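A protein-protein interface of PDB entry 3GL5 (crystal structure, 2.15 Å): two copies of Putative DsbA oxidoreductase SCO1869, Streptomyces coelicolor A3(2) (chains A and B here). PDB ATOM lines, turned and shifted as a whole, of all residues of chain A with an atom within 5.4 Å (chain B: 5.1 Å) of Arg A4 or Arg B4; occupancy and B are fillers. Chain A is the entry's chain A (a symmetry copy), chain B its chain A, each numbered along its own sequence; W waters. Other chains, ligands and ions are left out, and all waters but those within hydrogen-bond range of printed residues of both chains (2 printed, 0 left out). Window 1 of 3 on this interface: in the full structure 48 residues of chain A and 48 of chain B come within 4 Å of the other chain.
Arg B4 touches just one residue of chain A: Arg A4. Of the printed residues of chain B, His A2 touches Arg B191 (3.3 Å). Printed residues of chain A within 4 Å of Arg B191: His A2 (3.3 Å) and Met A3 (3.6 Å). Printed residues of chain B within 4 Å of Met A3: Arg B191. Of the printed residues of chain A, Met B3 touches Arg A191 (3.6 Å). Of the printed residues of chain B, Arg A191 touches His B2 (3.3 Å) and Met B3 (3.6 Å). The nearest printed residue of chain B that does not touch His A2 is Arg B4 (7.6 Å).
Water W2 lies within hydrogen-bond range of OE1 of Glu A37, NH1 of Arg A4 and NH1 of Arg B4. Water W1 lies within hydrogen-bond range of OE1 of Glu B37 (3.2 Å), NH1 of Arg B4 (3.2 Å) and NH1 of Arg A4 (3.3 Å).
Among the printed residues, merely in contact across the chains: Arg A191 with Met B3 (3.6 Å) and Met A3 with Arg B191 (3.6 Å).
The backbone carbonyl oxygen (O) of His B2 is in hydrogen-bond range of the guanidinium group (NH1) of Arg A191 (3.3 Å). The guanidinium group (NH1) of Arg B191 is in hydrogen-bond range of the backbone carbonyl oxygen (O) of His A2, at 3.3 Å. NH2 of Arg A4 sits close to NE of Arg B4, 3.5 Å away.
His A2 touches Arg B191, and with the chains exchanged Arg A191 touches His B2. Met A3 touches Arg B191, and with the chains exchanged Arg A191 touches Met B3. Arg B4 touches its own counterpart, Arg A4. 12 positions are printed for both chains. Of the 5 pairs that touch across the chains among the printed residues, 5 have their exchanged pair printed and touching as well.
The backbone carbonyl oxygen of Met B3 sits at hydrogen-bond distance from the backbone NH of Glu B37 (3.0 Å). The guanidinium group of Arg B4 lies within salt-bridge range of the side-chain carboxylate of Glu B6 (3.7 Å). O of Arg B4 is in hydrogen-bond range of N of Asp B190 (2.8 Å). OE1 of Glu B6 lies within salt-bridge range of NE of Arg B191 (2.9 Å). The backbone carbonyl oxygen (O) of Met A3 sits at hydrogen-bond distance from the backbone NH (N) of Glu A37, 3.0 Å away. OE1 of Glu A6 is in salt-bridge range of NE of Arg A191 (2.9 Å).
Printed residues of chain A that touch a printed residue of chain B: His A2, Met A3, Arg A4 and Arg A191. Of the 12 printed residues of chain B, 4 touch a printed residue of chain A.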
ATOM      1  N   HIS A   2     -19.193 -16.577  12.940  1.00  0.00           N
ATOM      2  CA  HIS A   2     -19.083 -15.076  13.003  1.00  0.00           C
ATOM      3  C   HIS A   2     -18.887 -14.521  11.604  1.00  0.00           C
ATOM      4  O   HIS A   2     -19.319 -15.171  10.634  1.00  0.00           O
ATOM      5  CB  HIS A   2     -17.933 -14.698  13.879  1.00  0.00           C
ATOM      6  N   MET A   3     -18.229 -13.352  11.505  1.00  0.00           N
ATOM      7  CA  MET A   3     -17.874 -12.734  10.223  1.00  0.00           C
ATOM      8  C   MET A   3     -16.717 -11.756  10.384  1.00  0.00           C
ATOM      9  O   MET A   3     -16.448 -11.283  11.483  1.00  0.00           O
ATOM     10  CB  MET A   3     -19.083 -11.996   9.598  1.00  0.00           C
ATOM     11  CG  MET A   3     -19.537 -10.789  10.338  1.00  0.00           C
ATOM     12  SD  MET A   3     -20.987  -9.779   9.420  1.00  0.00           S
ATOM     13  CE  MET A   3     -20.968  -8.329  10.689  1.00  0.00           C
ATOM     14  N   ARG A   4     -16.057 -11.441   9.274  1.00  0.00           N
ATOM     15  CA  ARG A   4     -14.911 -10.531   9.288  1.00  0.00           C
ATOM     16  C   ARG A   4     -15.308  -9.171   8.695  1.00  0.00           C
ATOM     17  O   ARG A   4     -16.086  -9.117   7.743  1.00  0.00           O
ATOM     18  CB  ARG A   4     -13.742 -11.164   8.497  1.00  0.00           C
ATOM     19  CG  ARG A   4     -12.453 -10.389   8.602  1.00  0.00           C
ATOM     20  CD  ARG A   4     -11.270 -10.998   7.844  1.00  0.00           C
ATOM     21  NE  ARG A   4     -11.561 -11.427   6.470  1.00  0.00           N
ATOM     22  CZ  ARG A   4     -10.627 -11.648   5.542  1.00  0.00           C
ATOM     23  NH1 ARG A   4      -9.338 -11.427   5.838  1.00  0.00           N
ATOM     24  NH2 ARG A   4     -10.972 -12.074   4.316  1.00  0.00           N
ATOM     25  N   VAL A   5     -14.818  -8.095   9.301  1.00  0.00           N
ATOM     26  CA  VAL A   5     -14.892  -6.733   8.743  1.00  0.00           C
ATOM     27  C   VAL A   5     -13.459  -6.200   8.428  1.00  0.00           C
ATOM     28  O   VAL A   5     -12.639  -5.979   9.355  1.00  0.00           O
ATOM     29  CB  VAL A   5     -15.613  -5.737   9.709  1.00  0.00           C
ATOM     30  CG1 VAL A   5     -15.506  -4.304   9.183  1.00  0.00           C
ATOM     31  CG2 VAL A   5     -17.057  -6.123   9.883  1.00  0.00           C
ATOM     32  N   GLU A   6     -13.160  -6.009   7.137  1.00  0.00           N
ATOM     33  CA  GLU A   6     -11.862  -5.446   6.711  1.00  0.00           C
ATOM     34  C   GLU A   6     -11.962  -3.944   6.463  1.00  0.00           C
ATOM     35  O   GLU A   6     -12.935  -3.454   5.855  1.00  0.00           O
ATOM     36  CB  GLU A   6     -11.382  -6.119   5.448  1.00  0.00           C
ATOM     37  CG  GLU A   6     -11.370  -7.648   5.545  1.00  0.00           C
ATOM     38  CD  GLU A   6     -11.303  -8.301   4.206  1.00  0.00           C
ATOM     39  OE1 GLU A   6     -12.366  -8.559   3.605  1.00  0.00           O
ATOM     40  OE2 GLU A   6     -10.173  -8.504   3.723  1.00  0.00           O
ATOM     41  N   VAL A  36     -17.464 -10.732  15.637  1.00  0.00           N
ATOM     42  CA  VAL A  36     -16.897  -9.945  14.534  1.00  0.00           C
ATOM     43  C   VAL A  36     -15.381  -9.870  14.667  1.00  0.00           C
ATOM     44  O   VAL A  36     -14.877  -9.539  15.737  1.00  0.00           O
ATOM     45  CB  VAL A  36     -17.483  -8.516  14.496  1.00  0.00           C
ATOM     46  CG1 VAL A  36     -16.786  -7.645  13.386  1.00  0.00           C
ATOM     47  CG2 VAL A  36     -19.031  -8.544  14.328  1.00  0.00           C
ATOM     48  N   GLU A  37     -14.645 -10.171  13.595  1.00  0.00           N
ATOM     49  CA  GLU A  37     -13.203  -9.935  13.589  1.00  0.00           C
ATOM     50  C   GLU A  37     -12.897  -8.744  12.674  1.00  0.00           C
ATOM     51  O   GLU A  37     -13.364  -8.707  11.549  1.00  0.00           O
ATOM     52  CB  GLU A  37     -12.469 -11.149  13.062  1.00  0.00           C
ATOM     53  CG  GLU A  37     -10.991 -11.098  13.393  1.00  0.00           C
ATOM     54  CD  GLU A  37     -10.117 -11.904  12.444  1.00  0.00           C
ATOM     55  OE1 GLU A  37     -10.670 -12.613  11.551  1.00  0.00           O
ATOM     56  OE2 GLU A  37      -8.863 -11.832  12.614  1.00  0.00           O
ATOM     57  N   VAL A  38     -12.119  -7.782  13.176  1.00  0.00           N
ATOM     58  CA  VAL A  38     -11.749  -6.569  12.440  1.00  0.00           C
ATOM     59  C   VAL A  38     -10.295  -6.712  11.973  1.00  0.00           C
ATOM     60  O   VAL A  38      -9.409  -7.002  12.786  1.00  0.00           O
ATOM     61  CB  VAL A  38     -11.883  -5.328  13.332  1.00  0.00           C
ATOM     62  CG1 VAL A  38     -11.450  -4.052  12.586  1.00  0.00           C
ATOM     63  CG2 VAL A  38     -13.308  -5.203  13.832  1.00  0.00           C
ATOM     64  N   VAL A  39     -10.057  -6.545  10.674  1.00  0.00           N
ATOM     65  CA  VAL A  39      -8.726  -6.680  10.113  1.00  0.00           C
ATOM     66  C   VAL A  39      -8.425  -5.349   9.408  1.00  0.00           C
ATOM     67  O   VAL A  39      -9.237  -4.879   8.591  1.00  0.00           O
ATOM     68  CB  VAL A  39      -8.649  -7.867   9.107  1.00  0.00           C
ATOM     69  CG1 VAL A  39      -7.275  -7.882   8.332  1.00  0.00           C
ATOM     70  CG2 VAL A  39      -8.863  -9.187   9.813  1.00  0.00           C
ATOM     71  N   ARG A  41      -6.117  -2.939   6.897  1.00  0.00           N
ATOM     72  CA  ARG A  41      -5.590  -3.161   5.551  1.00  0.00           C
ATOM     73  C   ARG A  41      -4.983  -1.862   5.041  1.00  0.00           C
ATOM     74  O   ARG A  41      -5.517  -0.794   5.311  1.00  0.00           O
ATOM     75  CB  ARG A  41      -6.740  -3.491   4.619  1.00  0.00           C
ATOM     76  CG  ARG A  41      -7.399  -4.789   4.913  1.00  0.00           C
ATOM     77  CD  ARG A  41      -6.589  -5.794   4.228  1.00  0.00           C
ATOM     78  NE  ARG A  41      -7.299  -7.025   4.162  1.00  0.00           N
ATOM     79  CZ  ARG A  41      -7.004  -7.987   3.306  1.00  0.00           C
ATOM     80  NH1 ARG A  41      -6.011  -7.840   2.405  1.00  0.00           N
ATOM     81  NH2 ARG A  41      -7.724  -9.092   3.341  1.00  0.00           N
ATOM     82  N   VAL A 188     -15.377  -3.507   4.371  1.00  0.00           N
ATOM     83  CA  VAL A 188     -15.945  -4.624   3.666  1.00  0.00           C
ATOM     84  C   VAL A 188     -16.405  -5.590   4.739  1.00  0.00           C
ATOM     85  O   VAL A 188     -15.607  -6.087   5.538  1.00  0.00           O
ATOM     86  CB  VAL A 188     -14.953  -5.228   2.661  1.00  0.00           C
ATOM     87  CG1 VAL A 188     -15.522  -6.518   2.030  1.00  0.00           C
ATOM     88  CG2 VAL A 188     -14.631  -4.173   1.571  1.00  0.00           C
ATOM     89  N   LEU A 189     -17.713  -5.818   4.753  1.00  0.00           N
ATOM     90  CA  LEU A 189     -18.345  -6.583   5.816  1.00  0.00           C
ATOM     91  C   LEU A 189     -18.662  -7.918   5.226  1.00  0.00           C
ATOM     92  O   LEU A 189     -19.502  -8.015   4.325  1.00  0.00           O
ATOM     93  CB  LEU A 189     -19.605  -5.879   6.339  1.00  0.00           C
ATOM     94  CG  LEU A 189     -19.322  -4.557   7.047  1.00  0.00           C
ATOM     95  CD1 LEU A 189     -19.280  -3.389   6.056  1.00  0.00           C
ATOM     96  CD2 LEU A 189     -20.325  -4.279   8.131  1.00  0.00           C
ATOM     97  N   ASP A 190     -17.950  -8.938   5.694  1.00  0.00           N
ATOM     98  CA  ASP A 190     -18.213 -10.309   5.265  1.00  0.00           C
ATOM     99  C   ASP A 190     -18.006 -10.560   3.763  1.00  0.00           C
ATOM    100  O   ASP A 190     -18.666 -11.422   3.195  1.00  0.00           O
ATOM    101  CB  ASP A 190     -19.647 -10.708   5.618  1.00  0.00           C
ATOM    102  CG  ASP A 190     -19.818 -12.216   5.703  1.00  0.00           C
ATOM    103  OD1 ASP A 190     -18.807 -12.913   6.031  1.00  0.00           O
ATOM    104  OD2 ASP A 190     -20.945 -12.696   5.452  1.00  0.00           O
ATOM    105  N   ARG A 191     -17.101  -9.823   3.114  1.00  0.00           N
ATOM    106  CA  ARG A 191     -17.002  -9.881   1.646  1.00  0.00           C
ATOM    107  C   ARG A 191     -18.373  -9.826   0.901  1.00  0.00           C
ATOM    108  O   ARG A 191     -18.469 -10.312  -0.225  1.00  0.00           O
ATOM    109  CB  ARG A 191     -16.169 -11.098   1.196  1.00  0.00           C
ATOM    110  CG  ARG A 191     -14.653 -11.004   1.485  1.00  0.00           C
ATOM    111  CD  ARG A 191     -13.953 -10.073   0.485  1.00  0.00           C
ATOM    112  NE  ARG A 191     -12.622  -9.675   0.940  1.00  0.00           N
ATOM    113  CZ  ARG A 191     -11.490 -10.297   0.609  1.00  0.00           C
ATOM    114  NH1 ARG A 191     -11.523 -11.356  -0.195  1.00  0.00           N
ATOM    115  NH2 ARG A 191     -10.316  -9.872   1.085  1.00  0.00           N
ATOM    116  N   HIS B   2      -9.722 -10.764  -4.483  1.00  0.00           N
ATOM    117  CA  HIS B   2      -9.376 -12.217  -4.281  1.00  0.00           C
ATOM    118  C   HIS B   2     -10.396 -12.860  -3.360  1.00  0.00           C
ATOM    119  O   HIS B   2     -11.543 -12.379  -3.305  1.00  0.00           O
ATOM    120  CB  HIS B   2      -8.004 -12.325  -3.697  1.00  0.00           C
ATOM    121  N   MET B   3      -9.977 -13.913  -2.637  1.00  0.00           N
ATOM    122  CA  MET B   3     -10.809 -14.582  -1.631  1.00  0.00           C
ATOM    123  C   MET B   3      -9.954 -15.345  -0.627  1.00  0.00           C
ATOM    124  O   MET B   3      -8.803 -15.667  -0.904  1.00  0.00           O
ATOM    125  CB  MET B   3     -11.815 -15.558  -2.289  1.00  0.00           C
ATOM    126  CG  MET B   3     -11.206 -16.749  -2.940  1.00  0.00           C
ATOM    127  SD  MET B   3     -12.539 -18.056  -3.634  1.00  0.00           S
ATOM    128  CE  MET B   3     -11.208 -19.362  -4.121  1.00  0.00           C
ATOM    129  N   ARG B   4     -10.539 -15.653   0.527  1.00  0.00           N
ATOM    130  CA  ARG B   4      -9.827 -16.364   1.589  1.00  0.00           C
ATOM    131  C   ARG B   4     -10.314 -17.818   1.670  1.00  0.00           C
ATOM    132  O   ARG B   4     -11.500 -18.082   1.484  1.00  0.00           O
ATOM    133  CB  ARG B   4     -10.041 -15.629   2.933  1.00  0.00           C
ATOM    134  CG  ARG B   4      -9.203 -16.176   4.061  1.00  0.00           C
ATOM    135  CD  ARG B   4      -9.378 -15.459   5.402  1.00  0.00           C
ATOM    136  NE  ARG B   4     -10.770 -15.210   5.802  1.00  0.00           N
ATOM    137  CZ  ARG B   4     -11.150 -14.930   7.051  1.00  0.00           C
ATOM    138  NH1 ARG B   4     -10.235 -14.915   8.031  1.00  0.00           N
ATOM    139  NH2 ARG B   4     -12.440 -14.679   7.330  1.00  0.00           N
ATOM    140  N   VAL B   5      -9.384 -18.742   1.888  1.00  0.00           N
ATOM    141  CA  VAL B   5      -9.683 -20.144   2.228  1.00  0.00           C
ATOM    142  C   VAL B   5      -9.175 -20.470   3.668  1.00  0.00           C
ATOM    143  O   VAL B   5      -7.945 -20.471   3.929  1.00  0.00           O
ATOM    144  CB  VAL B   5      -9.044 -21.149   1.215  1.00  0.00           C
ATOM    145  CG1 VAL B   5      -9.217 -22.589   1.703  1.00  0.00           C
ATOM    146  CG2 VAL B   5      -9.655 -20.983  -0.149  1.00  0.00           C
ATOM    147  N   GLU B   6     -10.110 -20.729   4.591  1.00  0.00           N
ATOM    148  CA  GLU B   6      -9.758 -21.115   5.973  1.00  0.00           C
ATOM    149  C   GLU B   6      -9.781 -22.630   6.149  1.00  0.00           C
ATOM    150  O   GLU B   6     -10.698 -23.322   5.663  1.00  0.00           O
ATOM    151  CB  GLU B   6     -10.719 -20.494   6.957  1.00  0.00           C
ATOM    152  CG  GLU B   6     -10.872 -18.979   6.778  1.00  0.00           C
ATOM    153  CD  GLU B   6     -12.095 -18.451   7.447  1.00  0.00           C
ATOM    154  OE1 GLU B   6     -13.167 -18.421   6.811  1.00  0.00           O
ATOM    155  OE2 GLU B   6     -11.995 -18.116   8.643  1.00  0.00           O
ATOM    156  N   GLU B  37      -5.936 -16.279  -0.310  1.00  0.00           N
ATOM    157  CA  GLU B  37      -5.205 -16.283   0.955  1.00  0.00           C
ATOM    158  C   GLU B  37      -5.654 -17.489   1.787  1.00  0.00           C
ATOM    159  O   GLU B  37      -6.843 -17.703   1.953  1.00  0.00           O
ATOM    160  CB  GLU B  37      -5.495 -15.021   1.740  1.00  0.00           C
ATOM    161  CG  GLU B  37      -4.486 -14.805   2.850  1.00  0.00           C
ATOM    162  CD  GLU B  37      -5.007 -13.962   4.003  1.00  0.00           C
ATOM    163  OE1 GLU B  37      -6.155 -13.435   3.910  1.00  0.00           O
ATOM    164  OE2 GLU B  37      -4.241 -13.818   5.003  1.00  0.00           O
ATOM    165  N   VAL B  39      -5.649 -19.383   5.435  1.00  0.00           N
ATOM    166  CA  VAL B  39      -5.508 -19.090   6.850  1.00  0.00           C
ATOM    167  C   VAL B  39      -5.757 -20.416   7.585  1.00  0.00           C
ATOM    168  O   VAL B  39      -6.778 -21.082   7.339  1.00  0.00           O
ATOM    169  CB  VAL B  39      -6.524 -18.004   7.311  1.00  0.00           C
ATOM    170  CG1 VAL B  39      -6.527 -17.842   8.881  1.00  0.00           C
ATOM    171  CG2 VAL B  39      -6.230 -16.675   6.652  1.00  0.00           C
ATOM    172  N   ARG B  41      -6.414 -22.650  11.052  1.00  0.00           N
ATOM    173  CA  ARG B  41      -7.352 -22.471  12.159  1.00  0.00           C
ATOM    174  C   ARG B  41      -7.291 -23.699  13.057  1.00  0.00           C
ATOM    175  O   ARG B  41      -7.148 -24.809  12.561  1.00  0.00           O
ATOM    176  CB  ARG B  41      -8.764 -22.416  11.607  1.00  0.00           C
ATOM    177  CG  ARG B  41      -9.036 -21.217  10.774  1.00  0.00           C
ATOM    178  CD  ARG B  41      -9.393 -20.164  11.722  1.00  0.00           C
ATOM    179  NE  ARG B  41      -9.989 -19.073  11.031  1.00  0.00           N
ATOM    180  CZ  ARG B  41     -10.736 -18.159  11.626  1.00  0.00           C
ATOM    181  NH1 ARG B  41     -11.006 -18.229  12.945  1.00  0.00           N
ATOM    182  NH2 ARG B  41     -11.230 -17.183  10.887  1.00  0.00           N
ATOM    183  N   VAL B 188     -13.166 -23.795   4.302  1.00  0.00           N
ATOM    184  CA  VAL B 188     -14.225 -22.852   4.064  1.00  0.00           C
ATOM    185  C   VAL B 188     -13.678 -21.877   3.041  1.00  0.00           C
ATOM    186  O   VAL B 188     -12.684 -21.188   3.281  1.00  0.00           O
ATOM    187  CB  VAL B 188     -14.705 -22.193   5.366  1.00  0.00           C
ATOM    188  CG1 VAL B 188     -15.729 -21.073   5.075  1.00  0.00           C
ATOM    189  CG2 VAL B 188     -15.319 -23.280   6.287  1.00  0.00           C
ATOM    190  N   LEU B 189     -14.337 -21.859   1.889  1.00  0.00           N
ATOM    191  CA  LEU B 189     -13.851 -21.110   0.740  1.00  0.00           C
ATOM    192  C   LEU B 189     -14.723 -19.902   0.641  1.00  0.00           C
ATOM    193  O   LEU B 189     -15.922 -20.023   0.362  1.00  0.00           O
ATOM    194  CB  LEU B 189     -13.899 -21.953  -0.541  1.00  0.00           C
ATOM    195  CG  LEU B 189     -12.944 -23.143  -0.530  1.00  0.00           C
ATOM    196  CD1 LEU B 189     -13.590 -24.376   0.110  1.00  0.00           C
ATOM    197  CD2 LEU B 189     -12.453 -23.476  -1.912  1.00  0.00           C
ATOM    198  N   ASP B 190     -14.138 -18.743   0.925  1.00  0.00           N
ATOM    199  CA  ASP B 190     -14.852 -17.477   0.788  1.00  0.00           C
ATOM    200  C   ASP B 190     -16.084 -17.336   1.697  1.00  0.00           C
ATOM    201  O   ASP B 190     -17.029 -16.645   1.334  1.00  0.00           O
ATOM    202  CB  ASP B 190     -15.308 -17.280  -0.659  1.00  0.00           C
ATOM    203  CG  ASP B 190     -15.556 -15.816  -0.989  1.00  0.00           C
ATOM    204  OD1 ASP B 190     -14.895 -14.941  -0.347  1.00  0.00           O
ATOM    205  OD2 ASP B 190     -16.395 -15.547  -1.875  1.00  0.00           O
ATOM    206  N   ARG B 191     -16.086 -17.975   2.868  1.00  0.00           N
ATOM    207  CA  ARG B 191     -17.310 -18.038   3.684  1.00  0.00           C
ATOM    208  C   ARG B 191     -18.607 -18.378   2.885  1.00  0.00           C
ATOM    209  O   ARG B 191     -19.699 -18.020   3.322  1.00  0.00           O
ATOM    210  CB  ARG B 191     -17.487 -16.751   4.515  1.00  0.00           C
ATOM    211  CG  ARG B 191     -16.489 -16.576   5.683  1.00  0.00           C
ATOM    212  CD  ARG B 191     -16.861 -17.472   6.872  1.00  0.00           C
ATOM    213  NE  ARG B 191     -15.761 -17.610   7.825  1.00  0.00           N
ATOM    214  CZ  ARG B 191     -15.596 -16.849   8.907  1.00  0.00           C
ATOM    215  NH1 ARG B 191     -16.473 -15.887   9.185  1.00  0.00           N
ATOM    216  NH2 ARG B 191     -14.550 -17.037   9.717  1.00  0.00           N
HETATM  217  O   HOH W   1      -7.418 -13.986   6.762  1.00  0.00           O
HETATM  218  O   HOH W   2      -8.917 -12.010   8.983  1.00  0.00           O
